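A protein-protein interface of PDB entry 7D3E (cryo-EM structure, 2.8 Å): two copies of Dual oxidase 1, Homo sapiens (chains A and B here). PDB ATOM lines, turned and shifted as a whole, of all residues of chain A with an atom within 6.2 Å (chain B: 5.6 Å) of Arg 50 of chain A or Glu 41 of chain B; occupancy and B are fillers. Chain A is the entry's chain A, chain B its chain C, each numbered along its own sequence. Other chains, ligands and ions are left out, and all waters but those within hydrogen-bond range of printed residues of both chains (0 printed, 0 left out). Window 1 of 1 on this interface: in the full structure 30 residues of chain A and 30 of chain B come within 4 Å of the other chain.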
ATOM      1  N   GLU A  41      15.503   9.899  21.976  1.00  0.00           N
ATOM      2  CA  GLU A  41      14.174   9.903  21.370  1.00  0.00           C
ATOM      3  C   GLU A  41      14.122  11.095  20.418  1.00  0.00           C
ATOM      4  O   GLU A  41      13.706  12.192  20.791  1.00  0.00           O
ATOM      5  CB  GLU A  41      13.085   9.974  22.433  1.00  0.00           C
ATOM      6  CG  GLU A  41      13.014   8.754  23.337  1.00  0.00           C
ATOM      7  CD  GLU A  41      12.451   7.531  22.637  1.00  0.00           C
ATOM      8  OE1 GLU A  41      11.803   7.690  21.579  1.00  0.00           O
ATOM      9  OE2 GLU A  41      12.653   6.409  23.146  1.00  0.00           O
ATOM     10  N   ARG A  43      12.266  11.648  17.845  1.00  0.00           N
ATOM     11  CA  ARG A  43      10.939  12.058  17.408  1.00  0.00           C
ATOM     12  C   ARG A  43      10.172  12.843  18.463  1.00  0.00           C
ATOM     13  O   ARG A  43       9.099  13.374  18.154  1.00  0.00           O
ATOM     14  CB  ARG A  43      10.111  10.837  16.995  1.00  0.00           C
ATOM     15  CG  ARG A  43      10.613  10.128  15.750  1.00  0.00           C
ATOM     16  CD  ARG A  43       9.655   9.027  15.325  1.00  0.00           C
ATOM     17  NE  ARG A  43       8.312   9.541  15.070  1.00  0.00           N
ATOM     18  CZ  ARG A  43       7.875   9.933  13.878  1.00  0.00           C
ATOM     19  NH1 ARG A  43       8.675   9.869  12.822  1.00  0.00           N
ATOM     20  NH2 ARG A  43       6.637  10.389  13.739  1.00  0.00           N
ATOM     21  N   TRP A  44      10.685  12.927  19.689  1.00  0.00           N
ATOM     22  CA  TRP A  44       9.972  13.627  20.751  1.00  0.00           C
ATOM     23  C   TRP A  44       9.826  15.107  20.421  1.00  0.00           C
ATOM     24  O   TRP A  44      10.793  15.771  20.038  1.00  0.00           O
ATOM     25  CB  TRP A  44      10.703  13.454  22.082  1.00  0.00           C
ATOM     26  CG  TRP A  44      10.334  12.200  22.805  1.00  0.00           C
ATOM     27  CD1 TRP A  44       9.483  11.226  22.372  1.00  0.00           C
ATOM     28  CD2 TRP A  44      10.795  11.787  24.096  1.00  0.00           C
ATOM     29  NE1 TRP A  44       9.390  10.227  23.311  1.00  0.00           N
ATOM     30  CE2 TRP A  44      10.186  10.547  24.378  1.00  0.00           C
ATOM     31  CE3 TRP A  44      11.669  12.338  25.037  1.00  0.00           C
ATOM     32  CZ2 TRP A  44      10.420   9.855  25.564  1.00  0.00           C
ATOM     33  CZ3 TRP A  44      11.900  11.648  26.213  1.00  0.00           C
ATOM     34  CH2 TRP A  44      11.278  10.419  26.466  1.00  0.00           C
ATOM     35  N   SER A  46       8.636  16.479  17.941  1.00  0.00           N
ATOM     36  CA  SER A  46       8.807  16.819  16.541  1.00  0.00           C
ATOM     37  C   SER A  46       7.455  16.959  15.852  1.00  0.00           C
ATOM     38  O   SER A  46       6.425  16.488  16.341  1.00  0.00           O
ATOM     39  CB  SER A  46       9.651  15.761  15.830  1.00  0.00           C
ATOM     40  OG  SER A  46       8.962  14.525  15.780  1.00  0.00           O
ATOM     41  N   GLY A  48       4.475  16.186  13.557  1.00  0.00           N
ATOM     42  CA  GLY A  48       3.884  14.938  13.131  1.00  0.00           C
ATOM     43  C   GLY A  48       3.891  13.833  14.165  1.00  0.00           C
ATOM     44  O   GLY A  48       3.303  12.773  13.917  1.00  0.00           O
ATOM     45  N   SER A  49       4.534  14.040  15.311  1.00  0.00           N
ATOM     46  CA  SER A  49       4.586  13.008  16.333  1.00  0.00           C
ATOM     47  C   SER A  49       3.233  12.861  17.023  1.00  0.00           C
ATOM     48  O   SER A  49       2.407  13.780  17.040  1.00  0.00           O
ATOM     49  CB  SER A  49       5.668  13.324  17.367  1.00  0.00           C
ATOM     50  OG  SER A  49       5.291  14.423  18.179  1.00  0.00           O
ATOM     51  N   ARG A  50       3.013  11.682  17.598  1.00  0.00           N
ATOM     52  CA  ARG A  50       1.760  11.393  18.275  1.00  0.00           C
ATOM     53  C   ARG A  50       1.660  12.168  19.588  1.00  0.00           C
ATOM     54  O   ARG A  50       2.659  12.612  20.160  1.00  0.00           O
ATOM     55  CB  ARG A  50       1.623   9.893  18.544  1.00  0.00           C
ATOM     56  CG  ARG A  50       2.303   9.406  19.822  1.00  0.00           C
ATOM     57  CD  ARG A  50       3.821   9.441  19.717  1.00  0.00           C
ATOM     58  NE  ARG A  50       4.467   8.999  20.949  1.00  0.00           N
ATOM     59  CZ  ARG A  50       4.788   9.806  21.956  1.00  0.00           C
ATOM     60  NH1 ARG A  50       4.522  11.103  21.879  1.00  0.00           N
ATOM     61  NH2 ARG A  50       5.375   9.316  23.039  1.00  0.00           N
ATOM     62  N   LEU A  51       0.428  12.332  20.058  1.00  0.00           N
ATOM     63  CA  LEU A  51       0.170  12.963  21.343  1.00  0.00           C
ATOM     64  C   LEU A  51       0.209  11.927  22.460  1.00  0.00           C
ATOM     65  O   LEU A  51      -0.123  10.756  22.261  1.00  0.00           O
ATOM     66  CB  LEU A  51      -1.187  13.670  21.341  1.00  0.00           C
ATOM     67  CG  LEU A  51      -1.347  14.892  20.434  1.00  0.00           C
ATOM     68  CD1 LEU A  51      -2.698  15.554  20.662  1.00  0.00           C
ATOM     69  CD2 LEU A  51      -0.220  15.883  20.666  1.00  0.00           C
ATOM     70  N   GLN A  52       0.623  12.374  23.643  1.00  0.00           N
ATOM     71  CA  GLN A  52       0.643  11.514  24.815  1.00  0.00           C
ATOM     72  C   GLN A  52      -0.773  11.305  25.349  1.00  0.00           C
ATOM     73  O   GLN A  52      -1.729  11.969  24.941  1.00  0.00           O
ATOM     74  CB  GLN A  52       1.540  12.109  25.900  1.00  0.00           C
ATOM     75  CG  GLN A  52       2.984  11.639  25.842  1.00  0.00           C
ATOM     76  CD  GLN A  52       3.154  10.225  26.360  1.00  0.00           C
ATOM     77  OE1 GLN A  52       2.319   9.724  27.111  1.00  0.00           O
ATOM     78  NE2 GLN A  52       4.239   9.573  25.959  1.00  0.00           N
ATOM     79  N   ASP A 152      -1.669   9.157  14.109  1.00  0.00           N
ATOM     80  CA  ASP A 152      -0.408   8.463  13.872  1.00  0.00           C
ATOM     81  C   ASP A 152      -0.652   7.229  13.014  1.00  0.00           C
ATOM     82  O   ASP A 152      -1.418   6.345  13.421  1.00  0.00           O
ATOM     83  CB  ASP A 152       0.226   8.077  15.209  1.00  0.00           C
ATOM     84  CG  ASP A 152       1.665   7.609  15.069  1.00  0.00           C
ATOM     85  OD1 ASP A 152       2.188   7.585  13.936  1.00  0.00           O
ATOM     86  OD2 ASP A 152       2.278   7.268  16.102  1.00  0.00           O
ATOM     87  N   THR A 155      -0.800   3.562  14.497  1.00  0.00           N
ATOM     88  CA  THR A 155      -1.754   3.266  15.559  1.00  0.00           C
ATOM     89  C   THR A 155      -3.145   3.037  14.969  1.00  0.00           C
ATOM     90  O   THR A 155      -3.353   3.101  13.755  1.00  0.00           O
ATOM     91  CB  THR A 155      -1.791   4.399  16.588  1.00  0.00           C
ATOM     92  OG1 THR A 155      -2.292   5.591  15.969  1.00  0.00           O
ATOM     93  CG2 THR A 155      -0.399   4.673  17.140  1.00  0.00           C
ATOM     94  N   ASP A 164      -4.012   7.255  18.075  1.00  0.00           N
ATOM     95  CA  ASP A 164      -3.447   8.398  18.775  1.00  0.00           C
ATOM     96  C   ASP A 164      -3.367   9.576  17.812  1.00  0.00           C
ATOM     97  O   ASP A 164      -2.889   9.415  16.674  1.00  0.00           O
ATOM     98  CB  ASP A 164      -2.058   8.068  19.337  1.00  0.00           C
ATOM     99  CG  ASP A 164      -2.091   6.930  20.338  1.00  0.00           C
ATOM    100  OD1 ASP A 164      -3.083   6.829  21.090  1.00  0.00           O
ATOM    101  OD2 ASP A 164      -1.126   6.138  20.371  1.00  0.00           O
ATOM    102  N   PRO A 165      -3.825  10.759  18.212  1.00  0.00           N
ATOM    103  CA  PRO A 165      -3.733  11.923  17.326  1.00  0.00           C
ATOM    104  C   PRO A 165      -2.291  12.343  17.095  1.00  0.00           C
ATOM    105  O   PRO A 165      -1.416  12.153  17.943  1.00  0.00           O
ATOM    106  CB  PRO A 165      -4.513  13.006  18.081  1.00  0.00           C
ATOM    107  CG  PRO A 165      -4.440  12.589  19.511  1.00  0.00           C
ATOM    108  CD  PRO A 165      -4.451  11.089  19.503  1.00  0.00           C
ATOM    109  N   ALA A 166      -2.053  12.924  15.923  1.00  0.00           N
ATOM    110  CA  ALA A 166      -0.736  13.413  15.539  1.00  0.00           C
ATOM    111  C   ALA A 166      -0.700  14.930  15.659  1.00  0.00           C
ATOM    112  O   ALA A 166      -1.614  15.618  15.190  1.00  0.00           O
ATOM    113  CB  ALA A 166      -0.390  12.986  14.111  1.00  0.00           C
ATOM    114  N   ASN A 167       0.354  15.448  16.284  1.00  0.00           N
ATOM    115  CA  ASN A 167       0.513  16.886  16.457  1.00  0.00           C
ATOM    116  C   ASN A 167       1.135  17.479  15.199  1.00  0.00           C
ATOM    117  O   ASN A 167       2.216  17.058  14.777  1.00  0.00           O
ATOM    118  CB  ASN A 167       1.374  17.182  17.681  1.00  0.00           C
ATOM    119  CG  ASN A 167       1.382  18.652  18.046  1.00  0.00           C
ATOM    120  OD1 ASN A 167       0.591  19.436  17.524  1.00  0.00           O
ATOM    121  ND2 ASN A 167       2.275  19.033  18.953  1.00  0.00           N
ATOM    122  N   ASP A 315       9.449  12.449  28.969  1.00  0.00           N
ATOM    123  CA  ASP A 315       8.705  12.642  27.730  1.00  0.00           C
ATOM    124  C   ASP A 315       7.943  13.961  27.793  1.00  0.00           C
ATOM    125  O   ASP A 315       7.068  14.117  28.651  1.00  0.00           O
ATOM    126  CB  ASP A 315       7.742  11.483  27.498  1.00  0.00           C
ATOM    127  CG  ASP A 315       7.141  11.487  26.103  1.00  0.00           C
ATOM    128  OD1 ASP A 315       7.445  12.408  25.315  1.00  0.00           O
ATOM    129  OD2 ASP A 315       6.364  10.561  25.790  1.00  0.00           O
ATOM    130  N   SER A 317       5.958  15.233  25.343  1.00  0.00           N
ATOM    131  CA  SER A 317       4.949  15.304  24.296  1.00  0.00           C
ATOM    132  C   SER A 317       3.625  15.815  24.848  1.00  0.00           C
ATOM    133  O   SER A 317       3.254  15.529  25.991  1.00  0.00           O
ATOM    134  CB  SER A 317       4.755  13.930  23.654  1.00  0.00           C
ATOM    135  OG  SER A 317       5.966  13.453  23.096  1.00  0.00           O
ATOM    136  N   ILE A 318       2.916  16.588  24.025  1.00  0.00           N
ATOM    137  CA  ILE A 318       1.621  17.122  24.422  1.00  0.00           C
ATOM    138  C   ILE A 318       0.637  15.976  24.600  1.00  0.00           C
ATOM    139  O   ILE A 318       0.511  15.103  23.733  1.00  0.00           O
ATOM    140  CB  ILE A 318       1.117  18.130  23.377  1.00  0.00           C
ATOM    141  CG1 ILE A 318       2.126  19.266  23.196  1.00  0.00           C
ATOM    142  CG2 ILE A 318      -0.246  18.674  23.773  1.00  0.00           C
ATOM    143  CD1 ILE A 318       2.375  20.069  24.452  1.00  0.00           C
ATOM    144  N   ASN B  37       4.252  -2.216  28.793  1.00  0.00           N
ATOM    145  CA  ASN B  37       4.369  -1.792  30.183  1.00  0.00           C
ATOM    146  C   ASN B  37       4.101  -0.298  30.316  1.00  0.00           C
ATOM    147  O   ASN B  37       3.374   0.134  31.217  1.00  0.00           O
ATOM    148  CB  ASN B  37       5.755  -2.157  30.722  1.00  0.00           C
ATOM    149  CG  ASN B  37       5.870  -1.986  32.228  1.00  0.00           C
ATOM    150  OD1 ASN B  37       5.513  -0.947  32.782  1.00  0.00           O
ATOM    151  ND2 ASN B  37       6.377  -3.016  32.899  1.00  0.00           N
ATOM    152  N   ASN B  38       4.678   0.503  29.425  1.00  0.00           N
ATOM    153  CA  ASN B  38       4.374   1.925  29.351  1.00  0.00           C
ATOM    154  C   ASN B  38       3.228   2.144  28.372  1.00  0.00           C
ATOM    155  O   ASN B  38       3.153   1.487  27.330  1.00  0.00           O
ATOM    156  CB  ASN B  38       5.603   2.726  28.921  1.00  0.00           C
ATOM    157  CG  ASN B  38       5.406   4.221  29.069  1.00  0.00           C
ATOM    158  OD1 ASN B  38       4.869   4.880  28.178  1.00  0.00           O
ATOM    159  ND2 ASN B  38       5.840   4.766  30.200  1.00  0.00           N
ATOM    160  N   LEU B  39       2.331   3.072  28.718  1.00  0.00           N
ATOM    161  CA  LEU B  39       1.095   3.230  27.956  1.00  0.00           C
ATOM    162  C   LEU B  39       1.369   3.666  26.521  1.00  0.00           C
ATOM    163  O   LEU B  39       0.790   3.120  25.574  1.00  0.00           O
ATOM    164  CB  LEU B  39       0.173   4.231  28.652  1.00  0.00           C
ATOM    165  CG  LEU B  39      -1.139   4.522  27.917  1.00  0.00           C
ATOM    166  CD1 LEU B  39      -1.933   3.240  27.707  1.00  0.00           C
ATOM    167  CD2 LEU B  39      -1.964   5.549  28.674  1.00  0.00           C
ATOM    168  N   MET B  40       2.252   4.647  26.336  1.00  0.00           N
ATOM    169  CA  MET B  40       2.479   5.220  25.018  1.00  0.00           C
ATOM    170  C   MET B  40       3.786   4.789  24.373  1.00  0.00           C
ATOM    171  O   MET B  40       3.922   4.912  23.152  1.00  0.00           O
ATOM    172  CB  MET B  40       2.439   6.753  25.093  1.00  0.00           C
ATOM    173  CG  MET B  40       1.102   7.299  25.561  1.00  0.00           C
ATOM    174  SD  MET B  40      -0.260   6.835  24.477  1.00  0.00           S
ATOM    175  CE  MET B  40       0.267   7.585  22.940  1.00  0.00           C
ATOM    176  N   GLU B  41       4.743   4.295  25.150  1.00  0.00           N
ATOM    177  CA  GLU B  41       6.007   3.781  24.631  1.00  0.00           C
ATOM    178  C   GLU B  41       6.019   2.278  24.894  1.00  0.00           C
ATOM    179  O   GLU B  41       6.515   1.814  25.922  1.00  0.00           O
ATOM    180  CB  GLU B  41       7.196   4.484  25.276  1.00  0.00           C
ATOM    181  CG  GLU B  41       7.298   5.964  24.949  1.00  0.00           C
ATOM    182  CD  GLU B  41       7.742   6.222  23.519  1.00  0.00           C
ATOM    183  OE1 GLU B  41       8.290   5.296  22.885  1.00  0.00           O
ATOM    184  OE2 GLU B  41       7.540   7.354  23.031  1.00  0.00           O
ATOM    185  N   HIS B  42       5.466   1.518  23.948  1.00  0.00           N
ATOM    186  CA  HIS B  42       5.297   0.083  24.142  1.00  0.00           C
ATOM    187  C   HIS B  42       6.609  -0.684  24.047  1.00  0.00           C
ATOM    188  O   HIS B  42       6.679  -1.821  24.524  1.00  0.00           O
ATOM    189  CB  HIS B  42       4.294  -0.462  23.125  1.00  0.00           C
ATOM    190  CG  HIS B  42       2.933   0.154  23.235  1.00  0.00           C
ATOM    191  ND1 HIS B  42       2.063   0.234  22.170  1.00  0.00           N
ATOM    192  CD2 HIS B  42       2.295   0.719  24.287  1.00  0.00           C
ATOM    193  CE1 HIS B  42       0.946   0.823  22.561  1.00  0.00           C
ATOM    194  NE2 HIS B  42       1.062   1.126  23.841  1.00  0.00           N
ATOM    195  N   ARG B  43       7.643  -0.097  23.448  1.00  0.00           N
ATOM    196  CA  ARG B  43       8.939  -0.754  23.342  1.00  0.00           C
ATOM    197  C   ARG B  43       9.836  -0.515  24.549  1.00  0.00           C
ATOM    198  O   ARG B  43      10.896  -1.144  24.643  1.00  0.00           O
ATOM    199  CB  ARG B  43       9.671  -0.292  22.077  1.00  0.00           C
ATOM    200  CG  ARG B  43       9.022  -0.735  20.779  1.00  0.00           C
ATOM    201  CD  ARG B  43       9.887  -0.367  19.584  1.00  0.00           C
ATOM    202  NE  ARG B  43      11.220  -0.956  19.675  1.00  0.00           N
ATOM    203  CZ  ARG B  43      11.557  -2.128  19.145  1.00  0.00           C
ATOM    204  NH1 ARG B  43      10.659  -2.842  18.482  1.00  0.00           N
ATOM    205  NH2 ARG B  43      12.796  -2.585  19.278  1.00  0.00           N
ATOM    206  N   TRP B  44       9.447   0.372  25.464  1.00  0.00           N
ATOM    207  CA  TRP B  44      10.287   0.673  26.616  1.00  0.00           C
ATOM    208  C   TRP B  44      10.464  -0.558  27.495  1.00  0.00           C
ATOM    209  O   TRP B  44       9.494  -1.242  27.834  1.00  0.00           O
ATOM    210  CB  TRP B  44       9.680   1.817  27.429  1.00  0.00           C
ATOM    211  CG  TRP B  44      10.062   3.171  26.927  1.00  0.00           C
ATOM    212  CD1 TRP B  44      10.825   3.453  25.833  1.00  0.00           C
ATOM    213  CD2 TRP B  44       9.710   4.433  27.506  1.00  0.00           C
ATOM    214  NE1 TRP B  44      10.964   4.812  25.690  1.00  0.00           N
ATOM    215  CE2 TRP B  44      10.289   5.436  26.705  1.00  0.00           C
ATOM    216  CE3 TRP B  44       8.954   4.811  28.621  1.00  0.00           C
ATOM    217  CZ2 TRP B  44      10.139   6.792  26.985  1.00  0.00           C
ATOM    218  CZ3 TRP B  44       8.807   6.158  28.896  1.00  0.00           C
ATOM    219  CH2 TRP B  44       9.396   7.132  28.081  1.00  0.00           C
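OE2 of Glu 41 of chain A lies within hydrogen-bond range of NE1 of Trp 44 of chain B (3.4 Å).
NE1 of Trp 44 of chain A is in hydrogen-bond range of OE2 of Glu 41 of chain B, at 3.4 Å.
The guanidinium group (NH2) of Arg 50 of chain A lies within salt-bridge range of the side-chain carboxylate (OE2) of Glu 41 of chain B, 2.9 Å away.
NH2 of Arg 50 of chain A sits close to NE2 of Gln 52 of chain A, at 3.1 Å.
NH1 of Arg 50 of chain A lies within hydrogen-bond range of OG of Ser 317 of chain A (3.0 Å).
N of Leu 51 of chain A is in hydrogen-bond range of O of Pro 165 of chain A, at 2.8 Å.
The backbone NH of Asp 152 of chain A is in hydrogen-bond range of the backbone carbonyl oxygen of Asp 164 of chain A, 2.9 Å away.
The side-chain hydroxyl (OG1) of Thr 155 of chain A lies within hydrogen-bond range of the backbone NH (N) of Asp 164 of chain A, at 3.2 Å.
The side-chain amide oxygen (OD1) of Asn 38 of chain B lies within hydrogen-bond range of the backbone NH (N) of Met 40 of chain B, at 3.2 Å.
Trp 44 of chain B touches Trp 44 of chain A (CZ2 to CZ2, 3.4 Å).
Met 40 of chain B touches Leu 51 of chain A (CE to O, 3.3 Å).
Gln 52 of chain A touches Met 40 of chain B (OE1 to CG, 3.1 Å).
Met 40 of chain B touches Asp 164 of chain A (CE to OD2, 3.3 Å).
Printed residues of chain B within 4 Å of Glu 41 of chain A: Trp 44 (3.4 Å).
Printed residues of chain B within 4 Å of Trp 44 of chain A: Glu 41 and Trp 44.
Of chain B, only Glu 41 comes within 4 Å of Arg 50 of chain A.
Printed residues of chain B within 4 Å of Gln 52 of chain A: Met 40 (3.1 Å).
Ala 166 of chain A touches none of the printed residues of chain B.
Ser 317 of chain A touches none of the printed residues of chain B.
Of the printed residues of chain A, Trp 44 of chain B touches Glu 41 (3.4 Å) and Trp 44 (3.4 Å).
The nearest residue of chain B that does not touch Arg 50 of chain A is Met 40 of chain B (4.1 Å).
Of the 8 printed residues of chain B, 3 touch a printed residue of chain A.
Among the printed residues, 7 pairs touch across the chains.
Glu 41 of chain A touches Trp 44 of chain B, and with the chains exchanged Trp 44 of chain A touches Glu 41 of chain B.
Trp 44 of chain A touches its own counterpart, Trp 44 of chain B.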
